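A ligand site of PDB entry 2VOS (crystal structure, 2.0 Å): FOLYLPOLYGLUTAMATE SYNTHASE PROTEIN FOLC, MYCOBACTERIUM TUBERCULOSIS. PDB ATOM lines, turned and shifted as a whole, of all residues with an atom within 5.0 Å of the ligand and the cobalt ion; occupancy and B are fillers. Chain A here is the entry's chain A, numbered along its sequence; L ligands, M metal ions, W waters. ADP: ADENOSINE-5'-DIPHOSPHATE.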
ATOM      1  N   GLY A  71     -36.694 -22.741 -25.930  1.00  0.00           N
ATOM      2  CA  GLY A  71     -35.573 -22.477 -26.823  1.00  0.00           C
ATOM      3  C   GLY A  71     -34.530 -23.522 -26.570  1.00  0.00           C
ATOM      4  O   GLY A  71     -34.758 -24.433 -25.762  1.00  0.00           O
ATOM      5  N   THR A  72     -33.362 -23.405 -27.209  1.00  0.00           N
ATOM      6  CA  THR A  72     -32.337 -24.405 -27.026  1.00  0.00           C
ATOM      7  C   THR A  72     -31.262 -23.972 -26.084  1.00  0.00           C
ATOM      8  O   THR A  72     -30.806 -24.788 -25.276  1.00  0.00           O
ATOM      9  CB  THR A  72     -31.655 -24.786 -28.371  1.00  0.00           C
ATOM     10  OG1 THR A  72     -32.699 -25.252 -29.256  1.00  0.00           O
ATOM     11  CG2 THR A  72     -30.711 -25.951 -28.120  1.00  0.00           C
ATOM     12  N   ASN A  73     -30.769 -22.755 -26.219  1.00  0.00           N
ATOM     13  CA  ASN A  73     -29.733 -22.300 -25.301  1.00  0.00           C
ATOM     14  C   ASN A  73     -30.191 -20.963 -24.632  1.00  0.00           C
ATOM     15  O   ASN A  73     -30.844 -20.161 -25.263  1.00  0.00           O
ATOM     16  CB  ASN A  73     -28.440 -22.016 -26.037  1.00  0.00           C
ATOM     17  CG  ASN A  73     -27.666 -23.285 -26.410  1.00  0.00           C
ATOM     18  OD1 ASN A  73     -27.793 -23.749 -27.524  1.00  0.00           O
ATOM     19  ND2 ASN A  73     -26.823 -23.824 -25.476  1.00  0.00           N
ATOM     20  N   GLY A  74     -29.806 -20.772 -23.373  1.00  0.00           N
ATOM     21  CA  GLY A  74     -30.092 -19.550 -22.632  1.00  0.00           C
ATOM     22  C   GLY A  74     -31.438 -19.589 -21.908  1.00  0.00           C
ATOM     23  O   GLY A  74     -31.816 -18.569 -21.300  1.00  0.00           O
ATOM     24  N   LYS A  75     -32.188 -20.684 -21.940  1.00  0.00           N
ATOM     25  CA  LYS A  75     -33.504 -20.629 -21.258  1.00  0.00           C
ATOM     26  C   LYS A  75     -33.341 -20.298 -19.775  1.00  0.00           C
ATOM     27  O   LYS A  75     -34.039 -19.429 -19.243  1.00  0.00           O
ATOM     28  CB  LYS A  75     -34.367 -21.918 -21.327  1.00  0.00           C
ATOM     29  CG  LYS A  75     -34.812 -22.381 -22.782  1.00  0.00           C
ATOM     30  CD  LYS A  75     -35.667 -23.643 -22.689  1.00  0.00           C
ATOM     31  CE  LYS A  75     -34.827 -24.879 -22.248  1.00  0.00           C
ATOM     32  NZ  LYS A  75     -33.567 -25.054 -23.074  1.00  0.00           N
ATOM     33  N   THR A  76     -32.531 -21.094 -19.086  1.00  0.00           N
ATOM     34  CA  THR A  76     -32.350 -20.901 -17.630  1.00  0.00           C
ATOM     35  C   THR A  76     -31.773 -19.510 -17.342  1.00  0.00           C
ATOM     36  O   THR A  76     -32.231 -18.816 -16.421  1.00  0.00           O
ATOM     37  CB  THR A  76     -31.467 -22.020 -16.999  1.00  0.00           C
ATOM     38  OG1 THR A  76     -32.271 -23.193 -16.984  1.00  0.00           O
ATOM     39  CG2 THR A  76     -31.168 -21.656 -15.507  1.00  0.00           C
ATOM     40  N   SER A  77     -30.748 -19.134 -18.087  1.00  0.00           N
ATOM     41  CA  SER A  77     -30.155 -17.818 -17.829  1.00  0.00           C
ATOM     42  C   SER A  77     -31.191 -16.679 -18.058  1.00  0.00           C
ATOM     43  O   SER A  77     -31.276 -15.711 -17.275  1.00  0.00           O
ATOM     44  CB  SER A  77     -28.976 -17.590 -18.773  1.00  0.00           C
ATOM     45  OG  SER A  77     -27.839 -18.350 -18.413  1.00  0.00           O
ATOM     46  N   SER A  98     -35.046 -25.694 -15.012  1.00  0.00           N
ATOM     47  CA  SER A  98     -34.556 -27.044 -15.144  1.00  0.00           C
ATOM     48  C   SER A  98     -33.401 -27.061 -16.162  1.00  0.00           C
ATOM     49  O   SER A  98     -33.166 -26.084 -16.934  1.00  0.00           O
ATOM     50  CB  SER A  98     -35.666 -28.030 -15.524  1.00  0.00           C
ATOM     51  OG  SER A  98     -36.232 -27.569 -16.729  1.00  0.00           O
ATOM     52  N   PRO A  99     -32.571 -28.122 -16.056  1.00  0.00           N
ATOM     53  CA  PRO A  99     -32.602 -29.076 -14.950  1.00  0.00           C
ATOM     54  C   PRO A  99     -32.010 -28.404 -13.682  1.00  0.00           C
ATOM     55  O   PRO A  99     -31.559 -27.280 -13.771  1.00  0.00           O
ATOM     56  CB  PRO A  99     -31.680 -30.237 -15.422  1.00  0.00           C
ATOM     57  CG  PRO A  99     -31.081 -29.805 -16.734  1.00  0.00           C
ATOM     58  CD  PRO A  99     -31.494 -28.365 -17.034  1.00  0.00           C
ATOM     59  N   GLU A 174     -39.781 -21.993 -17.065  1.00  0.00           N
ATOM     60  CA  GLU A 174     -38.962 -22.527 -18.135  1.00  0.00           C
ATOM     61  C   GLU A 174     -39.537 -23.882 -18.600  1.00  0.00           C
ATOM     62  O   GLU A 174     -39.852 -24.736 -17.786  1.00  0.00           O
ATOM     63  CB  GLU A 174     -37.534 -22.753 -17.632  1.00  0.00           C
ATOM     64  CG  GLU A 174     -36.650 -23.483 -18.581  1.00  0.00           C
ATOM     65  CD  GLU A 174     -35.204 -23.644 -18.055  1.00  0.00           C
ATOM     66  OE1 GLU A 174     -34.869 -23.273 -16.909  1.00  0.00           O
ATOM     67  OE2 GLU A 174     -34.386 -24.164 -18.828  1.00  0.00           O
ATOM     68  N   PRO A 196     -32.550 -18.682 -28.543  1.00  0.00           N
ATOM     69  CA  PRO A 196     -31.996 -19.272 -29.778  1.00  0.00           C
ATOM     70  C   PRO A 196     -32.181 -20.756 -29.848  1.00  0.00           C
ATOM     71  O   PRO A 196     -31.911 -21.469 -28.903  1.00  0.00           O
ATOM     72  CB  PRO A 196     -30.504 -18.923 -29.711  1.00  0.00           C
ATOM     73  CG  PRO A 196     -30.568 -17.481 -28.938  1.00  0.00           C
ATOM     74  CD  PRO A 196     -31.552 -17.869 -27.822  1.00  0.00           C
ATOM     75  N   HIS A 297     -22.915 -14.124 -25.549  1.00  0.00           N
ATOM     76  CA  HIS A 297     -24.243 -14.742 -25.514  1.00  0.00           C
ATOM     77  C   HIS A 297     -25.090 -14.241 -24.354  1.00  0.00           C
ATOM     78  O   HIS A 297     -26.335 -14.159 -24.479  1.00  0.00           O
ATOM     79  CB  HIS A 297     -24.167 -16.255 -25.403  1.00  0.00           C
ATOM     80  CG  HIS A 297     -23.338 -16.754 -24.243  1.00  0.00           C
ATOM     81  ND1 HIS A 297     -21.964 -16.627 -24.220  1.00  0.00           N
ATOM     82  CD2 HIS A 297     -23.669 -17.486 -23.146  1.00  0.00           C
ATOM     83  CE1 HIS A 297     -21.496 -17.171 -23.102  1.00  0.00           C
ATOM     84  NE2 HIS A 297     -22.507 -17.756 -22.470  1.00  0.00           N
ATOM     85  N   GLN A 298     -24.458 -13.937 -23.217  1.00  0.00           N
ATOM     86  CA  GLN A 298     -25.246 -13.394 -22.104  1.00  0.00           C
ATOM     87  C   GLN A 298     -25.779 -11.950 -22.388  1.00  0.00           C
ATOM     88  O   GLN A 298     -26.773 -11.547 -21.847  1.00  0.00           O
ATOM     89  CB  GLN A 298     -24.493 -13.483 -20.766  1.00  0.00           C
ATOM     90  CG  GLN A 298     -24.193 -14.964 -20.368  1.00  0.00           C
ATOM     91  CD  GLN A 298     -25.445 -15.722 -19.941  1.00  0.00           C
ATOM     92  OE1 GLN A 298     -26.559 -15.222 -20.045  1.00  0.00           O
ATOM     93  NE2 GLN A 298     -25.260 -16.913 -19.391  1.00  0.00           N
ATOM     94  N   ASN A 301     -28.986 -12.784 -24.208  1.00  0.00           N
ATOM     95  CA  ASN A 301     -29.955 -13.260 -23.223  1.00  0.00           C
ATOM     96  C   ASN A 301     -30.483 -12.050 -22.419  1.00  0.00           C
ATOM     97  O   ASN A 301     -31.675 -11.967 -22.186  1.00  0.00           O
ATOM     98  CB  ASN A 301     -29.335 -14.252 -22.215  1.00  0.00           C
ATOM     99  CG  ASN A 301     -28.934 -15.571 -22.883  1.00  0.00           C
ATOM    100  OD1 ASN A 301     -29.399 -15.858 -23.996  1.00  0.00           O
ATOM    101  ND2 ASN A 301     -28.126 -16.381 -22.202  1.00  0.00           N
ATOM    102  N   SER A 335     -26.082 -16.683 -12.627  1.00  0.00           N
ATOM    103  CA  SER A 335     -26.476 -17.876 -13.406  1.00  0.00           C
ATOM    104  C   SER A 335     -25.462 -18.996 -13.050  1.00  0.00           C
ATOM    105  O   SER A 335     -24.465 -19.174 -13.717  1.00  0.00           O
ATOM    106  CB  SER A 335     -26.509 -17.578 -14.902  1.00  0.00           C
ATOM    107  OG  SER A 335     -27.159 -18.666 -15.601  1.00  0.00           O
ATOM    108  N   GLY A 337     -23.240 -22.108 -12.545  1.00  0.00           N
ATOM    109  CA  GLY A 337     -22.815 -23.123 -13.512  1.00  0.00           C
ATOM    110  C   GLY A 337     -22.816 -22.652 -14.933  1.00  0.00           C
ATOM    111  O   GLY A 337     -22.653 -23.491 -15.812  1.00  0.00           O
ATOM    112  N   ARG A 338     -23.014 -21.349 -15.220  1.00  0.00           N
ATOM    113  CA  ARG A 338     -22.791 -20.814 -16.600  1.00  0.00           C
ATOM    114  C   ARG A 338     -21.568 -19.886 -16.589  1.00  0.00           C
ATOM    115  O   ARG A 338     -21.601 -18.737 -16.094  1.00  0.00           O
ATOM    116  CB  ARG A 338     -24.024 -20.059 -17.144  1.00  0.00           C
ATOM    117  CG  ARG A 338     -25.177 -21.019 -17.598  1.00  0.00           C
ATOM    118  CD  ARG A 338     -25.560 -21.966 -16.478  1.00  0.00           C
ATOM    119  NE  ARG A 338     -26.776 -22.742 -16.734  1.00  0.00           N
ATOM    120  CZ  ARG A 338     -27.335 -23.608 -15.867  1.00  0.00           C
ATOM    121  NH1 ARG A 338     -26.807 -23.853 -14.666  1.00  0.00           N
ATOM    122  NH2 ARG A 338     -28.425 -24.257 -16.199  1.00  0.00           N
ATOM    123  N   LEU A 339     -20.454 -20.444 -17.075  1.00  0.00           N
ATOM    124  CA  LEU A 339     -19.163 -19.789 -17.033  1.00  0.00           C
ATOM    125  C   LEU A 339     -18.925 -19.146 -15.676  1.00  0.00           C
ATOM    126  O   LEU A 339     -18.635 -17.931 -15.572  1.00  0.00           O
ATOM    127  CB  LEU A 339     -19.097 -18.729 -18.122  1.00  0.00           C
ATOM    128  CG  LEU A 339     -18.042 -18.711 -19.253  1.00  0.00           C
ATOM    129  CD1 LEU A 339     -16.905 -19.661 -19.149  1.00  0.00           C
ATOM    130  CD2 LEU A 339     -18.772 -18.681 -20.593  1.00  0.00           C
ATOM    131  N   ASP A 351     -19.073 -24.819 -16.379  1.00  0.00           N
ATOM    132  CA  ASP A 351     -19.994 -24.424 -17.411  1.00  0.00           C
ATOM    133  C   ASP A 351     -20.840 -25.613 -17.857  1.00  0.00           C
ATOM    134  O   ASP A 351     -20.310 -26.688 -18.167  1.00  0.00           O
ATOM    135  CB  ASP A 351     -19.283 -23.771 -18.596  1.00  0.00           C
ATOM    136  CG  ASP A 351     -20.293 -23.070 -19.534  1.00  0.00           C
ATOM    137  OD1 ASP A 351     -20.756 -21.962 -19.271  1.00  0.00           O
ATOM    138  OD2 ASP A 351     -20.705 -23.671 -20.497  1.00  0.00           O
ATOM    139  N   ALA A 352     -22.160 -25.406 -17.911  1.00  0.00           N
ATOM    140  CA  ALA A 352     -23.110 -26.449 -18.230  1.00  0.00           C
ATOM    141  C   ALA A 352     -23.138 -26.794 -19.752  1.00  0.00           C
ATOM    142  O   ALA A 352     -23.949 -27.649 -20.153  1.00  0.00           O
ATOM    143  CB  ALA A 352     -24.519 -26.022 -17.806  1.00  0.00           C
ATOM    144  N   ALA A 353     -22.311 -26.154 -20.592  1.00  0.00           N
ATOM    145  CA  ALA A 353     -22.385 -26.390 -22.039  1.00  0.00           C
ATOM    146  C   ALA A 353     -22.513 -27.875 -22.357  1.00  0.00           C
ATOM    147  O   ALA A 353     -21.722 -28.700 -21.887  1.00  0.00           O
ATOM    148  CB  ALA A 353     -21.166 -25.820 -22.745  1.00  0.00           C
ATOM    149  N   HIS A 354     -23.508 -28.219 -23.168  1.00  0.00           N
ATOM    150  CA  HIS A 354     -23.781 -29.615 -23.491  1.00  0.00           C
ATOM    151  C   HIS A 354     -24.349 -29.726 -24.929  1.00  0.00           C
ATOM    152  O   HIS A 354     -25.047 -30.728 -25.275  1.00  0.00           O
ATOM    153  CB  HIS A 354     -24.739 -30.241 -22.489  1.00  0.00           C
ATOM    154  CG  HIS A 354     -26.054 -29.549 -22.428  1.00  0.00           C
ATOM    155  ND1 HIS A 354     -26.343 -28.616 -21.465  1.00  0.00           N
ATOM    156  CD2 HIS A 354     -27.129 -29.622 -23.226  1.00  0.00           C
ATOM    157  CE1 HIS A 354     -27.565 -28.170 -21.646  1.00  0.00           C
ATOM    158  NE2 HIS A 354     -28.065 -28.763 -22.713  1.00  0.00           N
ATOM    159  N   ALA A 357     -23.693 -25.246 -30.018  1.00  0.00           N
ATOM    160  CA  ALA A 357     -23.877 -23.813 -29.783  1.00  0.00           C
ATOM    161  C   ALA A 357     -23.344 -23.333 -28.398  1.00  0.00           C
ATOM    162  O   ALA A 357     -22.660 -22.309 -28.338  1.00  0.00           O
ATOM    163  CB  ALA A 357     -25.325 -23.384 -29.955  1.00  0.00           C
ATOM    164  N   GLY A 358     -23.660 -24.053 -27.305  1.00  0.00           N
ATOM    165  CA  GLY A 358     -23.159 -23.669 -26.001  1.00  0.00           C
ATOM    166  C   GLY A 358     -21.634 -23.845 -25.881  1.00  0.00           C
ATOM    167  O   GLY A 358     -20.965 -23.005 -25.253  1.00  0.00           O
ATOM    168  N   ALA A 361     -20.092 -21.004 -27.554  1.00  0.00           N
ATOM    169  CA  ALA A 361     -20.208 -19.735 -26.781  1.00  0.00           C
ATOM    170  C   ALA A 361     -19.145 -19.723 -25.669  1.00  0.00           C
ATOM    171  O   ALA A 361     -18.450 -18.709 -25.447  1.00  0.00           O
ATOM    172  CB  ALA A 361     -21.579 -19.597 -26.184  1.00  0.00           C
ATOM    173  N   LEU A 362     -18.992 -20.875 -25.012  1.00  0.00           N
ATOM    174  CA  LEU A 362     -17.981 -21.074 -24.021  1.00  0.00           C
ATOM    175  C   LEU A 362     -16.558 -20.822 -24.579  1.00  0.00           C
ATOM    176  O   LEU A 362     -15.755 -20.079 -23.965  1.00  0.00           O
ATOM    177  CB  LEU A 362     -18.094 -22.501 -23.434  1.00  0.00           C
ATOM    178  CG  LEU A 362     -17.017 -22.992 -22.481  1.00  0.00           C
ATOM    179  CD1 LEU A 362     -16.775 -22.018 -21.257  1.00  0.00           C
ATOM    180  CD2 LEU A 362     -17.332 -24.459 -21.972  1.00  0.00           C
HETATM  181  PB  ADP L   1     -30.842 -23.757 -21.166  1.00  0.00           P
HETATM  182  O1B ADP L   1     -31.660 -23.515 -19.926  1.00  0.00           O
HETATM  183  O2B ADP L   1     -30.229 -25.132 -21.221  1.00  0.00           O
HETATM  184  O3B ADP L   1     -31.455 -23.335 -22.471  1.00  0.00           O
HETATM  185  PA  ADP L   1     -28.707 -22.139 -19.896  1.00  0.00           P
HETATM  186  O1A ADP L   1     -28.729 -23.142 -18.758  1.00  0.00           O
HETATM  187  O2A ADP L   1     -28.741 -20.624 -19.739  1.00  0.00           O
HETATM  188  O3A ADP L   1     -29.618 -22.685 -21.143  1.00  0.00           O
HETATM  189  O5' ADP L   1     -27.243 -22.389 -20.547  1.00  0.00           O
HETATM  190  C5' ADP L   1     -26.652 -23.683 -20.776  1.00  0.00           C
HETATM  191  C4' ADP L   1     -25.290 -23.400 -21.466  1.00  0.00           C
HETATM  192  O4' ADP L   1     -25.547 -22.815 -22.776  1.00  0.00           O
HETATM  193  C3' ADP L   1     -24.449 -22.322 -20.787  1.00  0.00           C
HETATM  194  O3' ADP L   1     -23.459 -22.894 -19.965  1.00  0.00           O
HETATM  195  C2' ADP L   1     -23.702 -21.563 -21.852  1.00  0.00           C
HETATM  196  O2' ADP L   1     -22.578 -22.422 -22.262  1.00  0.00           O
HETATM  197  C1' ADP L   1     -24.625 -21.712 -23.028  1.00  0.00           C
HETATM  198  N9  ADP L   1     -25.535 -20.566 -23.316  1.00  0.00           N
HETATM  199  C8  ADP L   1     -26.437 -19.895 -22.523  1.00  0.00           C
HETATM  200  N7  ADP L   1     -27.082 -18.945 -23.257  1.00  0.00           N
HETATM  201  C5  ADP L   1     -26.665 -19.095 -24.548  1.00  0.00           C
HETATM  202  C6  ADP L   1     -26.966 -18.470 -25.840  1.00  0.00           C
HETATM  203  N6  ADP L   1     -27.864 -17.467 -25.938  1.00  0.00           N
HETATM  204  N1  ADP L   1     -26.256 -18.902 -26.891  1.00  0.00           N
HETATM  205  C2  ADP L   1     -25.299 -19.859 -26.881  1.00  0.00           C
HETATM  206  N3  ADP L   1     -24.989 -20.524 -25.732  1.00  0.00           N
HETATM  207  C4  ADP L   1     -25.639 -20.146 -24.577  1.00  0.00           C
HETATM  208 CO    CO M   1     -32.342 -24.771 -18.499  1.00  0.00          CO
HETATM  209 MG    MG M   2     -29.946 -28.331 -23.396  1.00  0.00          MG
HETATM  210  O   HOH W   1     -25.384 -26.088 -23.866  1.00  0.00           O
HETATM  211  O   HOH W   2     -27.248 -15.615 -28.523  1.00  0.00           O
HETATM  212  O   HOH W   3     -29.127 -26.125 -23.565  1.00  0.00           O
HETATM  213  O   HOH W   4     -26.787 -18.536 -29.636  1.00  0.00           O
HETATM  214  O   HOH W   5     -29.748 -27.005 -19.682  1.00  0.00           O
HETATM  215  O   HOH W   6     -30.350 -25.317 -18.069  1.00  0.00           O
HETATM  216  O   HOH W   7     -32.571 -26.451 -19.829  1.00  0.00           O
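Water W6 lies within hydrogen-bond range of O1A of the ligand (2.8 Å) and NH2 of Arg 338 (2.9 Å).
Water W3 bridges O of Thr 72 (2.7 Å) and O2B of the ligand (2.8 Å).
Water W1 lies within hydrogen-bond range of the backbone NH (N) of His 354 (2.9 Å), the side-chain amide nitrogen (ND2) of Asn 73 (3.1 Å) and an oxygen (O4') of the ligand (3.5 Å).
The backbone NH of Thr 76 lies close to an oxygen (O1B) of the ligand.
N of Ser 77 is in hydrogen-bond range of O2A of the ligand (3.0 Å).
The side-chain hydroxyl (OG) of Ser 77 is in hydrogen-bond range of an oxygen (O2A) of the ligand, 2.8 Å away.
N of Lys 75 is in hydrogen-bond range of O3B of the ligand, 2.8 Å away.
The side-chain amino group (NZ) of Lys 75 lies within salt-bridge range of an oxygen (O3B) of the ligand (2.8 Å).
The guanidinium group of Arg 338 lies within salt-bridge range of an oxygen (O1A) of the ligand, 2.8 Å away.
OD2 of Asp 351 sits at hydrogen-bond distance from O2' of the ligand (2.9 Å).
O3A of the ligand is in hydrogen-bond range of N of Gly 74, 2.9 Å away.
OD1 of Asn 301 sits at hydrogen-bond distance from N6 of the ligand, 3.0 Å away.
An oxygen (O4') of the ligand lies within hydrogen-bond range of the side-chain amide nitrogen (ND2) of Asn 73 (3.2 Å).
The backbone carbonyl oxygen (O) of Gly 358 sits at hydrogen-bond distance from an oxygen (O2') of the ligand, 3.4 Å away.
O3' of the ligand is in hydrogen-bond range of N of Ala 352 (3.5 Å).
The cobalt ion is bound by O1B of the ligand, water W6, water W7, OE2 of Glu 174, OG1 of Thr 76 and O of Ser 98.
The backbone carbonyl oxygen (O) of Thr 72 lies close to an oxygen (O3B) of the ligand, 3.2 Å away.
CB of His 297 touches C6 of the ligand (3.6 Å).
N of Ala 353 touches O3' of the ligand, at 3.5 Å.
O of Ala 357 touches C2 of the ligand, at 3.9 Å.
Ala 361 touches the ligand.
Hydrophobic or aromatic side chains within 4 Å of the ligand: His 297, Ala 352, Ala 353 and Ala 361.
Of the 26 residues printed, 16 come within 4 Å of the ligand.
NE2 of Gln 298 lies within hydrogen-bond range of OG of Ser 77 (3.1 Å).
OG of Ser 77 lies within hydrogen-bond range of OG of Ser 335, 2.9 Å away.
OD2 of Asp 351 lies within hydrogen-bond range of N of Ala 353 (3.0 Å).
The side-chain carboxylate (OD1) of Asp 351 lies within hydrogen-bond range of the backbone NH (N) of Leu 339 (2.7 Å).
ND2 of Asn 301 sits at hydrogen-bond distance from OE1 of Gln 298, at 2.9 Å.
The backbone NH (N) of Asn 73 lies within hydrogen-bond range of the backbone carbonyl oxygen (O) of Pro 196 (3.2 Å).
The backbone carbonyl oxygen of Pro 196 lies within hydrogen-bond range of the backbone NH of Thr 72.
N of Ala 352 lies within hydrogen-bond range of O of Gly 337 (2.9 Å).
Residues that only touch the cobalt ion: Pro 99.
Of the 26 residues printed, 4 come within 4 Å of the cobalt ion.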
